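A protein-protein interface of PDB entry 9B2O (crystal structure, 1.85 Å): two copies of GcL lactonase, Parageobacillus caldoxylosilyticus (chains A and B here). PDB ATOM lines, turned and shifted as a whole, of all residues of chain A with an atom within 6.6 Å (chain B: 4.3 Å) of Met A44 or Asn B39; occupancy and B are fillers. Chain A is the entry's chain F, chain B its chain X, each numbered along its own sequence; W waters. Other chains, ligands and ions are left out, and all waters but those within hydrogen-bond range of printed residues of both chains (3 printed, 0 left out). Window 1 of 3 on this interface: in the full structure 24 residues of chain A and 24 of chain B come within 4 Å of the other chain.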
ATOM      1  N   LYS A  38      23.676  -3.708  -7.654  1.00  0.00           N
ATOM      2  CA  LYS A  38      23.343  -2.537  -6.822  1.00  0.00           C
ATOM      3  C   LYS A  38      23.257  -1.278  -7.701  1.00  0.00           C
ATOM      4  O   LYS A  38      22.591  -0.313  -7.266  1.00  0.00           O
ATOM      5  CB  LYS A  38      24.383  -2.298  -5.729  1.00  0.00           C
ATOM      6  CG  LYS A  38      23.902  -1.398  -4.589  1.00  0.00           C
ATOM      7  CD  LYS A  38      25.024  -1.100  -3.614  1.00  0.00           C
ATOM      8  CE  LYS A  38      24.827   0.090  -2.693  1.00  0.00           C
ATOM      9  NZ  LYS A  38      23.574  -0.006  -1.926  1.00  0.00           N
ATOM     10  N   ASN A  39      23.957  -1.236  -8.835  1.00  0.00           N
ATOM     11  CA  ASN A  39      23.884  -0.068  -9.777  1.00  0.00           C
ATOM     12  C   ASN A  39      22.458   0.151 -10.298  1.00  0.00           C
ATOM     13  O   ASN A  39      22.180   1.285 -10.647  1.00  0.00           O
ATOM     14  CB  ASN A  39      24.865  -0.150 -10.941  1.00  0.00           C
ATOM     15  CG  ASN A  39      26.280   0.125 -10.499  1.00  0.00           C
ATOM     16  OD1 ASN A  39      27.205  -0.632 -10.814  1.00  0.00           O
ATOM     17  ND2 ASN A  39      26.454   1.193  -9.765  1.00  0.00           N
ATOM     18  N   ILE A  42      21.059   2.028  -6.929  1.00  0.00           N
ATOM     19  CA  ILE A  42      21.760   3.315  -6.677  1.00  0.00           C
ATOM     20  C   ILE A  42      22.742   3.580  -7.843  1.00  0.00           C
ATOM     21  O   ILE A  42      23.818   2.911  -7.909  1.00  0.00           O
ATOM     22  CB  ILE A  42      22.461   3.273  -5.293  1.00  0.00           C
ATOM     23  CG1 ILE A  42      21.530   2.910  -4.127  1.00  0.00           C
ATOM     24  CG2 ILE A  42      23.155   4.575  -5.033  1.00  0.00           C
ATOM     25  CD1 ILE A  42      20.459   3.971  -3.816  1.00  0.00           C
ATOM     26  N   ALA A  43      22.375   4.457  -8.790  1.00  0.00           N
ATOM     27  CA  ALA A  43      23.178   4.742 -10.010  1.00  0.00           C
ATOM     28  C   ALA A  43      24.601   5.119  -9.597  1.00  0.00           C
ATOM     29  O   ALA A  43      24.751   5.953  -8.665  1.00  0.00           O
ATOM     30  CB  ALA A  43      22.572   5.858 -10.834  1.00  0.00           C
ATOM     31  N   MET A  44      25.603   4.540 -10.264  1.00  0.00           N
ATOM     32  CA  MET A  44      27.028   4.919 -10.100  1.00  0.00           C
ATOM     33  C   MET A  44      27.389   4.918  -8.619  1.00  0.00           C
ATOM     34  O   MET A  44      27.992   5.860  -8.159  1.00  0.00           O
ATOM     35  CB  MET A  44      27.276   6.301 -10.702  1.00  0.00           C
ATOM     36  CG  MET A  44      26.875   6.356 -12.154  1.00  0.00           C
ATOM     37  SD  MET A  44      27.721   5.180 -13.244  1.00  0.00           S
ATOM     38  CE  MET A  44      29.399   5.415 -12.646  1.00  0.00           C
ATOM     39  N   HIS A  45      27.036   3.864  -7.893  1.00  0.00           N
ATOM     40  CA  HIS A  45      27.212   3.831  -6.427  1.00  0.00           C
ATOM     41  C   HIS A  45      28.690   3.724  -6.079  1.00  0.00           C
ATOM     42  O   HIS A  45      29.002   4.105  -4.963  1.00  0.00           O
ATOM     43  CB  HIS A  45      26.431   2.684  -5.767  1.00  0.00           C
ATOM     44  CG  HIS A  45      27.063   1.342  -5.926  1.00  0.00           C
ATOM     45  ND1 HIS A  45      27.755   0.713  -4.885  1.00  0.00           N
ATOM     46  CD2 HIS A  45      27.085   0.485  -6.972  1.00  0.00           C
ATOM     47  CE1 HIS A  45      28.189  -0.471  -5.310  1.00  0.00           C
ATOM     48  NE2 HIS A  45      27.778  -0.638  -6.585  1.00  0.00           N
ATOM     49  N   ASN A  46      29.539   3.195  -6.971  1.00  0.00           N
ATOM     50  CA  ASN A  46      30.981   2.939  -6.662  1.00  0.00           C
ATOM     51  C   ASN A  46      31.816   3.118  -7.934  1.00  0.00           C
ATOM     52  O   ASN A  46      32.295   2.142  -8.521  1.00  0.00           O
ATOM     53  CB  ASN A  46      31.143   1.565  -6.003  1.00  0.00           C
ATOM     54  CG  ASN A  46      32.585   1.251  -5.682  1.00  0.00           C
ATOM     55  OD1 ASN A  46      33.344   2.140  -5.309  1.00  0.00           O
ATOM     56  ND2 ASN A  46      32.991   0.022  -5.935  1.00  0.00           N
ATOM     57  N   PRO A  47      31.962   4.364  -8.447  1.00  0.00           N
ATOM     58  CA  PRO A  47      32.560   4.568  -9.766  1.00  0.00           C
ATOM     59  C   PRO A  47      34.042   4.160  -9.770  1.00  0.00           C
ATOM     60  O   PRO A  47      34.712   4.360  -8.773  1.00  0.00           O
ATOM     61  CB  PRO A  47      32.440   6.076 -10.021  1.00  0.00           C
ATOM     62  CG  PRO A  47      31.416   6.569  -8.987  1.00  0.00           C
ATOM     63  CD  PRO A  47      31.559   5.628  -7.806  1.00  0.00           C
ATOM     64  N   ALA A  48      34.493   3.616 -10.891  1.00  0.00           N
ATOM     65  CA  ALA A  48      35.915   3.374 -11.204  1.00  0.00           C
ATOM     66  C   ALA A  48      36.734   4.662 -11.029  1.00  0.00           C
ATOM     67  O   ALA A  48      36.253   5.794 -11.341  1.00  0.00           O
ATOM     68  CB  ALA A  48      36.038   2.801 -12.596  1.00  0.00           C
ATOM     69  N   ALA A  55      36.608  -1.363 -11.002  1.00  0.00           N
ATOM     70  CA  ALA A  55      35.731  -1.388  -9.807  1.00  0.00           C
ATOM     71  C   ALA A  55      34.609  -2.412  -9.995  1.00  0.00           C
ATOM     72  O   ALA A  55      34.036  -2.553 -11.112  1.00  0.00           O
ATOM     73  CB  ALA A  55      35.188  -0.023  -9.485  1.00  0.00           C
ATOM     74  N   PRO A 248      19.321   8.613  -7.153  1.00  0.00           N
ATOM     75  CA  PRO A 248      18.428   7.955  -8.094  1.00  0.00           C
ATOM     76  C   PRO A 248      18.908   6.587  -8.536  1.00  0.00           C
ATOM     77  O   PRO A 248      20.087   6.252  -8.409  1.00  0.00           O
ATOM     78  CB  PRO A 248      18.420   8.912  -9.295  1.00  0.00           C
ATOM     79  CG  PRO A 248      19.786   9.572  -9.230  1.00  0.00           C
ATOM     80  CD  PRO A 248      20.047   9.756  -7.749  1.00  0.00           C
ATOM     81  N   PRO A 249      17.991   5.762  -9.059  1.00  0.00           N
ATOM     82  CA  PRO A 249      18.343   4.458  -9.610  1.00  0.00           C
ATOM     83  C   PRO A 249      19.127   4.518 -10.938  1.00  0.00           C
ATOM     84  O   PRO A 249      19.161   5.574 -11.591  1.00  0.00           O
ATOM     85  CB  PRO A 249      16.960   3.798  -9.779  1.00  0.00           C
ATOM     86  CG  PRO A 249      16.010   4.949  -9.994  1.00  0.00           C
ATOM     87  CD  PRO A 249      16.538   6.018  -9.069  1.00  0.00           C
ATOM     88  N   GLY A 250      19.770   3.397 -11.285  1.00  0.00           N
ATOM     89  CA  GLY A 250      20.781   3.297 -12.369  1.00  0.00           C
ATOM     90  C   GLY A 250      20.154   3.350 -13.747  1.00  0.00           C
ATOM     91  O   GLY A 250      20.879   3.588 -14.757  1.00  0.00           O
ATOM     92  N   ASP B  37      35.015   5.637 -15.729  1.00  0.00           N
ATOM     93  CA  ASP B  37      34.170   4.423 -15.666  1.00  0.00           C
ATOM     94  C   ASP B  37      33.332   4.376 -16.929  1.00  0.00           C
ATOM     95  O   ASP B  37      32.666   5.395 -17.231  1.00  0.00           O
ATOM     96  CB  ASP B  37      33.351   4.470 -14.380  1.00  0.00           C
ATOM     97  CG  ASP B  37      32.654   3.204 -13.977  1.00  0.00           C
ATOM     98  OD1 ASP B  37      32.144   2.431 -14.883  1.00  0.00           O
ATOM     99  OD2 ASP B  37      32.540   3.033 -12.739  1.00  0.00           O
ATOM    100  N   LYS B  38      33.290   3.242 -17.620  1.00  0.00           N
ATOM    101  CA  LYS B  38      32.474   3.118 -18.848  1.00  0.00           C
ATOM    102  C   LYS B  38      30.976   3.253 -18.516  1.00  0.00           C
ATOM    103  O   LYS B  38      30.202   3.560 -19.435  1.00  0.00           O
ATOM    104  CB  LYS B  38      32.670   1.765 -19.531  1.00  0.00           C
ATOM    105  CG  LYS B  38      32.148   1.698 -20.970  1.00  0.00           C
ATOM    106  CD  LYS B  38      32.344   0.326 -21.605  1.00  0.00           C
ATOM    107  CE  LYS B  38      31.528   0.067 -22.861  1.00  0.00           C
ATOM    108  NZ  LYS B  38      31.797   1.071 -23.905  1.00  0.00           N
ATOM    109  N   ASN B  39      30.574   2.954 -17.284  1.00  0.00           N
ATOM    110  CA  ASN B  39      29.150   3.113 -16.840  1.00  0.00           C
ATOM    111  C   ASN B  39      28.703   4.581 -16.936  1.00  0.00           C
ATOM    112  O   ASN B  39      27.515   4.790 -17.109  1.00  0.00           O
ATOM    113  CB  ASN B  39      28.888   2.544 -15.447  1.00  0.00           C
ATOM    114  CG  ASN B  39      28.813   1.034 -15.438  1.00  0.00           C
ATOM    115  OD1 ASN B  39      29.459   0.378 -14.619  1.00  0.00           O
ATOM    116  ND2 ASN B  39      28.023   0.480 -16.329  1.00  0.00           N
ATOM    117  N   TRP B  40      29.593   5.561 -16.808  1.00  0.00           N
ATOM    118  CA  TRP B  40      29.257   6.980 -17.097  1.00  0.00           C
ATOM    119  C   TRP B  40      28.855   7.110 -18.569  1.00  0.00           C
ATOM    120  O   TRP B  40      28.009   7.975 -18.875  1.00  0.00           O
ATOM    121  CB  TRP B  40      30.388   7.965 -16.813  1.00  0.00           C
ATOM    122  CG  TRP B  40      30.861   8.088 -15.398  1.00  0.00           C
ATOM    123  CD1 TRP B  40      32.126   7.836 -14.953  1.00  0.00           C
ATOM    124  CD2 TRP B  40      30.152   8.618 -14.272  1.00  0.00           C
ATOM    125  NE1 TRP B  40      32.237   8.100 -13.618  1.00  0.00           N
ATOM    126  CE2 TRP B  40      31.048   8.614 -13.177  1.00  0.00           C
ATOM    127  CE3 TRP B  40      28.858   9.128 -14.085  1.00  0.00           C
ATOM    128  CZ2 TRP B  40      30.682   9.069 -11.907  1.00  0.00           C
ATOM    129  CZ3 TRP B  40      28.501   9.582 -12.835  1.00  0.00           C
ATOM    130  CH2 TRP B  40      29.385   9.515 -11.750  1.00  0.00           C
ATOM    131  N   MET B  41      29.558   6.412 -19.462  1.00  0.00           N
ATOM    132  CA  MET B  41      29.419   6.571 -20.929  1.00  0.00           C
ATOM    133  C   MET B  41      28.179   5.822 -21.412  1.00  0.00           C
ATOM    134  O   MET B  41      27.459   6.367 -22.277  1.00  0.00           O
ATOM    135  CB  MET B  41      30.655   6.007 -21.640  1.00  0.00           C
ATOM    136  CG  MET B  41      30.755   6.358 -23.106  1.00  0.00           C
ATOM    137  SD  MET B  41      31.848   7.795 -23.345  1.00  0.00           S
ATOM    138  CE  MET B  41      33.454   7.015 -23.262  1.00  0.00           C
ATOM    139  N   ILE B  42      28.005   4.592 -20.922  1.00  0.00           N
ATOM    140  CA  ILE B  42      26.951   3.625 -21.333  1.00  0.00           C
ATOM    141  C   ILE B  42      26.351   3.002 -20.057  1.00  0.00           C
ATOM    142  O   ILE B  42      26.984   2.092 -19.441  1.00  0.00           O
ATOM    143  CB  ILE B  42      27.513   2.575 -22.313  1.00  0.00           C
ATOM    144  CG1 ILE B  42      28.201   3.198 -23.536  1.00  0.00           C
ATOM    145  CG2 ILE B  42      26.421   1.599 -22.708  1.00  0.00           C
ATOM    146  CD1 ILE B  42      27.236   3.851 -24.522  1.00  0.00           C
ATOM    147  N   ALA B  43      25.204   3.525 -19.625  1.00  0.00           N
ATOM    148  CA  ALA B  43      24.482   3.093 -18.403  1.00  0.00           C
ATOM    149  C   ALA B  43      24.354   1.573 -18.393  1.00  0.00           C
ATOM    150  O   ALA B  43      23.897   1.027 -19.427  1.00  0.00           O
ATOM    151  CB  ALA B  43      23.116   3.729 -18.323  1.00  0.00           C
ATOM    152  N   MET B  44      24.748   0.928 -17.282  1.00  0.00           N
ATOM    153  CA  MET B  44      24.497  -0.521 -17.047  1.00  0.00           C
ATOM    154  C   MET B  44      25.023  -1.337 -18.217  1.00  0.00           C
ATOM    155  O   MET B  44      24.318  -2.229 -18.705  1.00  0.00           O
ATOM    156  CB  MET B  44      23.001  -0.787 -16.861  1.00  0.00           C
ATOM    157  CG  MET B  44      22.398  -0.021 -15.722  1.00  0.00           C
ATOM    158  SD  MET B  44      23.174  -0.231 -14.065  1.00  0.00           S
ATOM    159  CE  MET B  44      23.266  -2.025 -14.059  1.00  0.00           C
ATOM    160  N   HIS B  45      26.245  -1.045 -18.659  1.00  0.00           N
ATOM    161  CA  HIS B  45      26.828  -1.685 -19.858  1.00  0.00           C
ATOM    162  C   HIS B  45      27.103  -3.157 -19.581  1.00  0.00           C
ATOM    163  O   HIS B  45      27.186  -3.877 -20.558  1.00  0.00           O
ATOM    164  CB  HIS B  45      28.104  -0.975 -20.332  1.00  0.00           C
ATOM    165  CG  HIS B  45      29.327  -1.300 -19.553  1.00  0.00           C
ATOM    166  ND1 HIS B  45      30.274  -2.195 -20.017  1.00  0.00           N
ATOM    167  CD2 HIS B  45      29.800  -0.817 -18.386  1.00  0.00           C
ATOM    168  CE1 HIS B  45      31.273  -2.260 -19.143  1.00  0.00           C
ATOM    169  NE2 HIS B  45      31.013  -1.420 -18.137  1.00  0.00           N
ATOM    170  N   THR B  57      33.623  -3.217 -13.946  1.00  0.00           N
ATOM    171  CA  THR B  57      33.572  -2.197 -15.013  1.00  0.00           C
ATOM    172  C   THR B  57      34.974  -2.081 -15.632  1.00  0.00           C
ATOM    173  O   THR B  57      35.886  -2.862 -15.253  1.00  0.00           O
ATOM    174  CB  THR B  57      33.007  -0.881 -14.467  1.00  0.00           C
ATOM    175  OG1 THR B  57      32.679  -0.072 -15.592  1.00  0.00           O
ATOM    176  CG2 THR B  57      33.959  -0.145 -13.554  1.00  0.00           C
ATOM    177  N   GLY B 250      25.280   6.919 -18.016  1.00  0.00           N
ATOM    178  CA  GLY B 250      25.021   6.310 -16.690  1.00  0.00           C
ATOM    179  C   GLY B 250      24.377   7.292 -15.730  1.00  0.00           C
ATOM    180  O   GLY B 250      23.788   6.874 -14.694  1.00  0.00           O
HETATM  181  O   HOH W   1      35.118   7.272 -13.380  1.00  0.00           O
HETATM  182  O   HOH W   2      25.554   2.873 -15.253  1.00  0.00           O
HETATM  183  O   HOH W   3      23.398   4.305 -14.317  1.00  0.00           O
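Water W3 lies within hydrogen-bond range of the backbone carbonyl oxygen of Gly B250 (2.6 Å) and the backbone carbonyl oxygen of Gly A250 (2.7 Å).
Water W1 lies within hydrogen-bond range of the backbone carbonyl oxygen (O) of Ala A48 (2.8 Å), the backbone NH (N) of Asp B37 (2.9 Å) and the indole nitrogen (NE1) of Trp B40 (3.0 Å).
Water W2 lies within hydrogen-bond range of N of Met B44, O of Asn B39 and SD of Met A44.
NE2 of His B45 sits at hydrogen-bond distance from OG1 of Thr B57, at 3.3 Å.
N of Met B44 lies close to ND2 of Asn B39 (3.4 Å).
The side-chain carboxylate (OD1) of Asp B37 lies within hydrogen-bond range of the side-chain hydroxyl (OG1) of Thr B57 (2.7 Å).
The backbone carbonyl oxygen of Trp B40 lies within hydrogen-bond range of the backbone NH of Gly B250, at 3.0 Å.
The side-chain carboxylate (OD1) of Asp B37 is in hydrogen-bond range of the backbone NH (N) of Asn B39 (2.9 Å).
ND2 of Asn B39 lies close to N of His B45 (3.3 Å).
OD2 of Asp B37 is in hydrogen-bond range of N of Ala A48 (2.8 Å).
The backbone NH (N) of Thr B57 is in hydrogen-bond range of the backbone carbonyl oxygen (O) of Ala A55 (2.9 Å).
Among the printed residues, merely in contact across the chains: Asn A39 with Met B44, Met A44 with Asp B37, Met A44 with Asn B39, Met A44 with Trp B40, Pro A47 with Asp B37, Pro A47 with Trp B40 and Ala A48 with Thr B57.
Hydrophobic or aromatic side chains of chain B that line the printed part of chain A: Trp B40 and Met B44.
Hydrophobic or aromatic side chains of chain A within 4 Å of the printed part of chain B: Met A44, Pro A47 and Ala A48.
Among the printed residues, no Asp or Glu carboxylate lies within 4 Å of a Lys or Arg side-chain nitrogen of the other chain.
Met A44 touches three residues of chain B.
Asn B39 touches one residue of chain A.
Of the printed residues of chain A, Thr B57 touches Ala A48 (3.7 Å) and Ala A55 (2.9 Å).
Of the printed residues of chain B, Ala A55 touches Thr B57.
Printed residues of chain A within 4 Å of Trp B40: Met A44 and Pro A47.
His A45 touches none of the printed residues of chain B.
Lys B38 touches none of the printed residues of chain A.
Asn A39 touches Met B44, and with the chains exchanged Met A44 touches Asn B39.
Positions printed for both chains: 38, 39, 42, 43, 44, 45 and 250.
Of the 9 pairs that touch across the chains among the printed residues, 2 have their exchanged pair printed and touching as well.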
